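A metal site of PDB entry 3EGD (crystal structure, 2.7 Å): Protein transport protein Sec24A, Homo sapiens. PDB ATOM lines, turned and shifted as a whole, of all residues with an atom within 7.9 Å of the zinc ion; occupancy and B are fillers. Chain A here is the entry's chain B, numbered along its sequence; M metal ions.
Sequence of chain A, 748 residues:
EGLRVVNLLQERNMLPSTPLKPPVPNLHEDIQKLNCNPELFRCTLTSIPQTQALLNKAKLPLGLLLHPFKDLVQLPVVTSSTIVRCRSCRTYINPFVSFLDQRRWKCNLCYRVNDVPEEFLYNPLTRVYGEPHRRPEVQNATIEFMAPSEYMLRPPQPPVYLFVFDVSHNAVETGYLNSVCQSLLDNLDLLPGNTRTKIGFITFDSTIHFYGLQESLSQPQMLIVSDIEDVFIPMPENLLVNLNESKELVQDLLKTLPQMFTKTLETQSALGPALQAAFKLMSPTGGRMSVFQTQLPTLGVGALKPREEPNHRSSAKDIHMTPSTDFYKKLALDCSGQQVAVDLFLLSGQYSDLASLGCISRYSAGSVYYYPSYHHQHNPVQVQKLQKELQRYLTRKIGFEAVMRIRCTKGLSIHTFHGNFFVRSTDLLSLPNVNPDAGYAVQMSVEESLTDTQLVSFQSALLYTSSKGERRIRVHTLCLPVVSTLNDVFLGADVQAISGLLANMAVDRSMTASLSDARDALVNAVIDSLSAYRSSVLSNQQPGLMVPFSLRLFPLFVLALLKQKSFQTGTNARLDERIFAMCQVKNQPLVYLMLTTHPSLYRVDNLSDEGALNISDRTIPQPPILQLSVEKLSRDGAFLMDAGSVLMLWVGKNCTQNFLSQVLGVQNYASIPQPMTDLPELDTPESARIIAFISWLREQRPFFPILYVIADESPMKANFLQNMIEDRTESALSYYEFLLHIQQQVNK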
ATOM      1  N   ARG A  85     -15.702  19.657   2.507  1.00  0.00           N
ATOM      2  CA  ARG A  85     -15.270  19.661   1.102  1.00  0.00           C
ATOM      3  C   ARG A  85     -15.579  18.341   0.399  1.00  0.00           C
ATOM      4  O   ARG A  85     -15.362  17.272   0.962  1.00  0.00           O
ATOM      5  CB  ARG A  85     -13.766  19.907   1.016  1.00  0.00           C
ATOM      6  CG  ARG A  85     -13.224  20.968   1.954  1.00  0.00           C
ATOM      7  CD  ARG A  85     -11.722  21.139   1.744  1.00  0.00           C
ATOM      8  NE  ARG A  85     -11.414  21.576   0.393  1.00  0.00           N
ATOM      9  CZ  ARG A  85     -10.182  21.800  -0.066  1.00  0.00           C
ATOM     10  NH1 ARG A  85      -9.137  21.628   0.730  1.00  0.00           N
ATOM     11  NH2 ARG A  85      -9.993  22.181  -1.321  1.00  0.00           N
ATOM     12  N   CYS A  86     -16.073  18.413  -0.834  1.00  0.00           N
ATOM     13  CA  CYS A  86     -16.394  17.193  -1.579  1.00  0.00           C
ATOM     14  C   CYS A  86     -15.230  16.210  -1.538  1.00  0.00           C
ATOM     15  O   CYS A  86     -14.086  16.594  -1.769  1.00  0.00           O
ATOM     16  CB  CYS A  86     -16.717  17.524  -3.034  1.00  0.00           C
ATOM     17  SG  CYS A  86     -16.443  16.128  -4.129  1.00  0.00           S
ATOM     18  N   ARG A  87     -15.535  14.941  -1.263  1.00  0.00           N
ATOM     19  CA  ARG A  87     -14.492  13.925  -1.170  1.00  0.00           C
ATOM     20  C   ARG A  87     -13.800  13.560  -2.476  1.00  0.00           C
ATOM     21  O   ARG A  87     -12.791  12.867  -2.458  1.00  0.00           O
ATOM     22  CB  ARG A  87     -15.072  12.657  -0.535  1.00  0.00           C
ATOM     23  CG  ARG A  87     -15.325  12.756   0.970  1.00  0.00           C
ATOM     24  CD  ARG A  87     -15.791  11.417   1.524  1.00  0.00           C
ATOM     25  NE  ARG A  87     -16.115  11.469   2.948  1.00  0.00           N
ATOM     26  CZ  ARG A  87     -16.695  10.487   3.627  1.00  0.00           C
ATOM     27  NH1 ARG A  87     -17.021   9.362   2.998  1.00  0.00           N
ATOM     28  NH2 ARG A  87     -16.956  10.620   4.914  1.00  0.00           N
ATOM     29  N   SER A  88     -14.338  14.009  -3.601  1.00  0.00           N
ATOM     30  CA  SER A  88     -13.714  13.678  -4.876  1.00  0.00           C
ATOM     31  C   SER A  88     -12.871  14.829  -5.405  1.00  0.00           C
ATOM     32  O   SER A  88     -11.646  14.751  -5.399  1.00  0.00           O
ATOM     33  CB  SER A  88     -14.777  13.325  -5.919  1.00  0.00           C
ATOM     34  OG  SER A  88     -15.405  12.084  -5.624  1.00  0.00           O
ATOM     35  N   CYS A  89     -13.532  15.884  -5.854  1.00  0.00           N
ATOM     36  CA  CYS A  89     -12.861  17.048  -6.424  1.00  0.00           C
ATOM     37  C   CYS A  89     -12.419  18.071  -5.372  1.00  0.00           C
ATOM     38  O   CYS A  89     -11.776  19.073  -5.698  1.00  0.00           O
ATOM     39  CB  CYS A  89     -13.792  17.728  -7.411  1.00  0.00           C
ATOM     40  SG  CYS A  89     -15.224  18.412  -6.571  1.00  0.00           S
ATOM     41  N   ARG A  90     -12.794  17.828  -4.123  1.00  0.00           N
ATOM     42  CA  ARG A  90     -12.419  18.702  -3.018  1.00  0.00           C
ATOM     43  C   ARG A  90     -12.943  20.129  -3.058  1.00  0.00           C
ATOM     44  O   ARG A  90     -12.341  21.023  -2.485  1.00  0.00           O
ATOM     45  CB  ARG A  90     -10.888  18.739  -2.874  1.00  0.00           C
ATOM     46  CG  ARG A  90     -10.290  17.404  -2.487  1.00  0.00           C
ATOM     47  CD  ARG A  90     -10.979  16.880  -1.225  1.00  0.00           C
ATOM     48  NE  ARG A  90     -10.210  17.071  -0.001  1.00  0.00           N
ATOM     49  CZ  ARG A  90     -10.759  17.249   1.201  1.00  0.00           C
ATOM     50  NH1 ARG A  90     -12.079  17.278   1.328  1.00  0.00           N
ATOM     51  NH2 ARG A  90      -9.988  17.361   2.277  1.00  0.00           N
ATOM     52  N   THR A  91     -14.070  20.332  -3.725  1.00  0.00           N
ATOM     53  CA  THR A  91     -14.699  21.645  -3.793  1.00  0.00           C
ATOM     54  C   THR A  91     -15.305  22.011  -2.432  1.00  0.00           C
ATOM     55  O   THR A  91     -15.806  21.151  -1.710  1.00  0.00           O
ATOM     56  CB  THR A  91     -15.795  21.643  -4.868  1.00  0.00           C
ATOM     57  OG1 THR A  91     -15.178  21.545  -6.161  1.00  0.00           O
ATOM     58  CG2 THR A  91     -16.650  22.896  -4.789  1.00  0.00           C
ATOM     59  N   TYR A  92     -15.264  23.293  -2.072  1.00  0.00           N
ATOM     60  CA  TYR A  92     -15.797  23.728  -0.782  1.00  0.00           C
ATOM     61  C   TYR A  92     -17.333  23.789  -0.739  1.00  0.00           C
ATOM     62  O   TYR A  92     -17.957  24.378  -1.620  1.00  0.00           O
ATOM     63  CB  TYR A  92     -15.237  25.101  -0.396  1.00  0.00           C
ATOM     64  CG  TYR A  92     -13.736  25.109  -0.182  1.00  0.00           C
ATOM     65  CD1 TYR A  92     -13.180  24.726   1.041  1.00  0.00           C
ATOM     66  CD2 TYR A  92     -12.869  25.459  -1.224  1.00  0.00           C
ATOM     67  CE1 TYR A  92     -11.791  24.689   1.218  1.00  0.00           C
ATOM     68  CE2 TYR A  92     -11.486  25.427  -1.054  1.00  0.00           C
ATOM     69  CZ  TYR A  92     -10.959  25.048   0.169  1.00  0.00           C
ATOM     70  OH  TYR A  92      -9.595  24.998   0.322  1.00  0.00           O
ATOM     71  N   TRP A 105     -25.157  15.855   0.605  1.00  0.00           N
ATOM     72  CA  TRP A 105     -25.185  16.976  -0.334  1.00  0.00           C
ATOM     73  C   TRP A 105     -24.583  16.632  -1.686  1.00  0.00           C
ATOM     74  O   TRP A 105     -23.615  15.882  -1.788  1.00  0.00           O
ATOM     75  CB  TRP A 105     -24.452  18.187   0.254  1.00  0.00           C
ATOM     76  CG  TRP A 105     -23.003  17.936   0.554  1.00  0.00           C
ATOM     77  CD1 TRP A 105     -22.488  17.199   1.586  1.00  0.00           C
ATOM     78  CD2 TRP A 105     -21.879  18.425  -0.189  1.00  0.00           C
ATOM     79  NE1 TRP A 105     -21.122  17.198   1.529  1.00  0.00           N
ATOM     80  CE2 TRP A 105     -20.721  17.949   0.451  1.00  0.00           C
ATOM     81  CE3 TRP A 105     -21.749  19.217  -1.337  1.00  0.00           C
ATOM     82  CZ2 TRP A 105     -19.432  18.242  -0.013  1.00  0.00           C
ATOM     83  CZ3 TRP A 105     -20.471  19.503  -1.797  1.00  0.00           C
ATOM     84  CH2 TRP A 105     -19.329  19.022  -1.130  1.00  0.00           C
ATOM     85  N   LYS A 106     -25.168  17.194  -2.736  1.00  0.00           N
ATOM     86  CA  LYS A 106     -24.687  16.961  -4.084  1.00  0.00           C
ATOM     87  C   LYS A 106     -23.722  18.076  -4.493  1.00  0.00           C
ATOM     88  O   LYS A 106     -24.121  19.240  -4.609  1.00  0.00           O
ATOM     89  CB  LYS A 106     -25.857  16.879  -5.061  1.00  0.00           C
ATOM     90  CG  LYS A 106     -25.441  16.945  -6.527  1.00  0.00           C
ATOM     91  CD  LYS A 106     -26.600  16.613  -7.454  1.00  0.00           C
ATOM     92  CE  LYS A 106     -26.957  15.152  -7.388  1.00  0.00           C
ATOM     93  NZ  LYS A 106     -28.061  14.804  -8.317  1.00  0.00           N
ATOM     94  N   CYS A 107     -22.459  17.719  -4.717  1.00  0.00           N
ATOM     95  CA  CYS A 107     -21.447  18.688  -5.130  1.00  0.00           C
ATOM     96  C   CYS A 107     -21.787  19.258  -6.500  1.00  0.00           C
ATOM     97  O   CYS A 107     -21.896  18.515  -7.479  1.00  0.00           O
ATOM     98  CB  CYS A 107     -20.073  18.035  -5.192  1.00  0.00           C
ATOM     99  SG  CYS A 107     -18.836  19.121  -5.949  1.00  0.00           S
ATOM    100  N   ASN A 108     -21.947  20.581  -6.573  1.00  0.00           N
ATOM    101  CA  ASN A 108     -22.297  21.233  -7.818  1.00  0.00           C
ATOM    102  C   ASN A 108     -21.175  21.308  -8.852  1.00  0.00           C
ATOM    103  O   ASN A 108     -21.356  21.894  -9.915  1.00  0.00           O
ATOM    104  CB  ASN A 108     -22.853  22.637  -7.539  1.00  0.00           C
ATOM    105  CG  ASN A 108     -21.829  23.554  -6.894  1.00  0.00           C
ATOM    106  OD1 ASN A 108     -20.920  23.105  -6.189  1.00  0.00           O
ATOM    107  ND2 ASN A 108     -21.983  24.857  -7.113  1.00  0.00           N
ATOM    108  N   LEU A 109     -20.026  20.712  -8.548  1.00  0.00           N
ATOM    109  CA  LEU A 109     -18.937  20.736  -9.514  1.00  0.00           C
ATOM    110  C   LEU A 109     -18.617  19.380 -10.149  1.00  0.00           C
ATOM    111  O   LEU A 109     -18.332  19.328 -11.346  1.00  0.00           O
ATOM    112  CB  LEU A 109     -17.675  21.365  -8.891  1.00  0.00           C
ATOM    113  CG  LEU A 109     -17.592  22.880  -9.099  1.00  0.00           C
ATOM    114  CD1 LEU A 109     -18.739  23.597  -8.388  1.00  0.00           C
ATOM    115  CD2 LEU A 109     -16.271  23.399  -8.593  1.00  0.00           C
ATOM    116  N   CYS A 110     -18.669  18.293  -9.373  1.00  0.00           N
ATOM    117  CA  CYS A 110     -18.398  16.970  -9.944  1.00  0.00           C
ATOM    118  C   CYS A 110     -19.585  16.008  -9.715  1.00  0.00           C
ATOM    119  O   CYS A 110     -19.498  14.813 -10.011  1.00  0.00           O
ATOM    120  CB  CYS A 110     -17.103  16.374  -9.388  1.00  0.00           C
ATOM    121  SG  CYS A 110     -17.234  15.427  -7.859  1.00  0.00           S
ATOM    122  N   TYR A 111     -20.673  16.561  -9.191  1.00  0.00           N
ATOM    123  CA  TYR A 111     -21.932  15.838  -8.944  1.00  0.00           C
ATOM    124  C   TYR A 111     -21.942  14.769  -7.864  1.00  0.00           C
ATOM    125  O   TYR A 111     -23.025  14.380  -7.405  1.00  0.00           O
ATOM    126  CB  TYR A 111     -22.452  15.231 -10.243  1.00  0.00           C
ATOM    127  CG  TYR A 111     -22.513  16.204 -11.402  1.00  0.00           C
ATOM    128  CD1 TYR A 111     -23.279  17.364 -11.331  1.00  0.00           C
ATOM    129  CD2 TYR A 111     -21.776  15.965 -12.559  1.00  0.00           C
ATOM    130  CE1 TYR A 111     -23.306  18.269 -12.385  1.00  0.00           C
ATOM    131  CE2 TYR A 111     -21.790  16.864 -13.614  1.00  0.00           C
ATOM    132  CZ  TYR A 111     -22.562  18.010 -13.534  1.00  0.00           C
ATOM    133  OH  TYR A 111     -22.585  18.892 -14.596  1.00  0.00           O
ATOM    134  N   ARG A 112     -20.785  14.281  -7.460  1.00  0.00           N
ATOM    135  CA  ARG A 112     -20.763  13.268  -6.406  1.00  0.00           C
ATOM    136  C   ARG A 112     -21.557  13.718  -5.189  1.00  0.00           C
ATOM    137  O   ARG A 112     -21.660  14.916  -4.909  1.00  0.00           O
ATOM    138  CB  ARG A 112     -19.333  12.932  -5.982  1.00  0.00           C
ATOM    139  CG  ARG A 112     -19.285  12.247  -4.610  1.00  0.00           C
ATOM    140  CD  ARG A 112     -18.000  11.495  -4.337  1.00  0.00           C
ATOM    141  NE  ARG A 112     -18.002  10.983  -2.966  1.00  0.00           N
ATOM    142  CZ  ARG A 112     -17.096  10.162  -2.457  1.00  0.00           C
ATOM    143  NH1 ARG A 112     -16.076   9.715  -3.205  1.00  0.00           N
ATOM    144  NH2 ARG A 112     -17.191   9.777  -1.196  1.00  0.00           N
ATOM    145  N   VAL A 113     -22.129  12.758  -4.462  1.00  0.00           N
ATOM    146  CA  VAL A 113     -22.896  13.056  -3.268  1.00  0.00           C
ATOM    147  C   VAL A 113     -22.046  12.805  -2.031  1.00  0.00           C
ATOM    148  O   VAL A 113     -21.391  11.767  -1.922  1.00  0.00           O
ATOM    149  CB  VAL A 113     -24.152  12.161  -3.179  1.00  0.00           C
ATOM    150  CG1 VAL A 113     -25.061  12.638  -2.046  1.00  0.00           C
ATOM    151  CG2 VAL A 113     -24.883  12.174  -4.513  1.00  0.00           C
ATOM    152  N   ASN A 114     -22.047  13.759  -1.112  1.00  0.00           N
ATOM    153  CA  ASN A 114     -21.260  13.643   0.116  1.00  0.00           C
ATOM    154  C   ASN A 114     -22.115  13.613   1.378  1.00  0.00           C
ATOM    155  O   ASN A 114     -23.303  13.950   1.355  1.00  0.00           O
ATOM    156  CB  ASN A 114     -20.272  14.809   0.200  1.00  0.00           C
ATOM    157  CG  ASN A 114     -19.109  14.660  -0.771  1.00  0.00           C
ATOM    158  OD1 ASN A 114     -18.117  13.987  -0.491  1.00  0.00           O
ATOM    159  ND2 ASN A 114     -19.229  15.296  -1.931  1.00  0.00           N
ATOM    160  N   ARG A 407     -11.729  26.280  -9.445  1.00  0.00           N
ATOM    161  CA  ARG A 407     -12.352  25.044  -9.841  1.00  0.00           C
ATOM    162  C   ARG A 407     -13.604  25.430 -10.597  1.00  0.00           C
ATOM    163  O   ARG A 407     -14.223  26.450 -10.294  1.00  0.00           O
ATOM    164  CB  ARG A 407     -12.737  24.224  -8.606  1.00  0.00           C
ATOM    165  CG  ARG A 407     -11.593  23.495  -7.912  1.00  0.00           C
ATOM    166  CD  ARG A 407     -12.167  22.564  -6.826  1.00  0.00           C
ATOM    167  NE  ARG A 407     -11.125  21.859  -6.093  1.00  0.00           N
ATOM    168  CZ  ARG A 407     -10.326  22.431  -5.191  1.00  0.00           C
ATOM    169  NH1 ARG A 407     -10.458  23.714  -4.900  1.00  0.00           N
ATOM    170  NH2 ARG A 407      -9.390  21.703  -4.601  1.00  0.00           N
HETATM  171 ZN    ZN M   1     -17.330  17.368  -6.170  1.00  0.00          ZN
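N of Leu 109 sits close to SG of Cys 107 (3.3 Å).
N of Cys 107 sits at hydrogen-bond distance from O of Arg 112 (2.9 Å).
The side-chain sulfur (SG) of Cys 89 lies close to the side-chain hydroxyl (OG1) of Thr 91 (3.2 Å).
NE of Arg 407 lies within hydrogen-bond range of O of Cys 89 (2.9 Å).
The backbone NH of Cys 86 sits at hydrogen-bond distance from the backbone carbonyl oxygen of Thr 91 (2.9 Å).
The backbone NH (N) of Ser 88 lies close to the side-chain sulfur (SG) of Cys 86, at 3.0 Å.
The side-chain sulfur (SG) of Cys 86 lies close to the side-chain amide nitrogen (ND2) of Asn 114.
The backbone NH (N) of Arg 112 sits close to the side-chain sulfur (SG) of Cys 110, 3.8 Å away.
Along chain A the residues within 4 Å of the zinc ion span positions 86 to 110.
The nearest printed residue that does not touch the zinc ion is Tyr 111 (4.6 Å).
The zinc ion is bound by SG of Cys 107 (2.3 Å), SG of Cys 89 (2.4 Å), SG of Cys 86 (2.5 Å) and SG of Cys 110 (2.6 Å).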
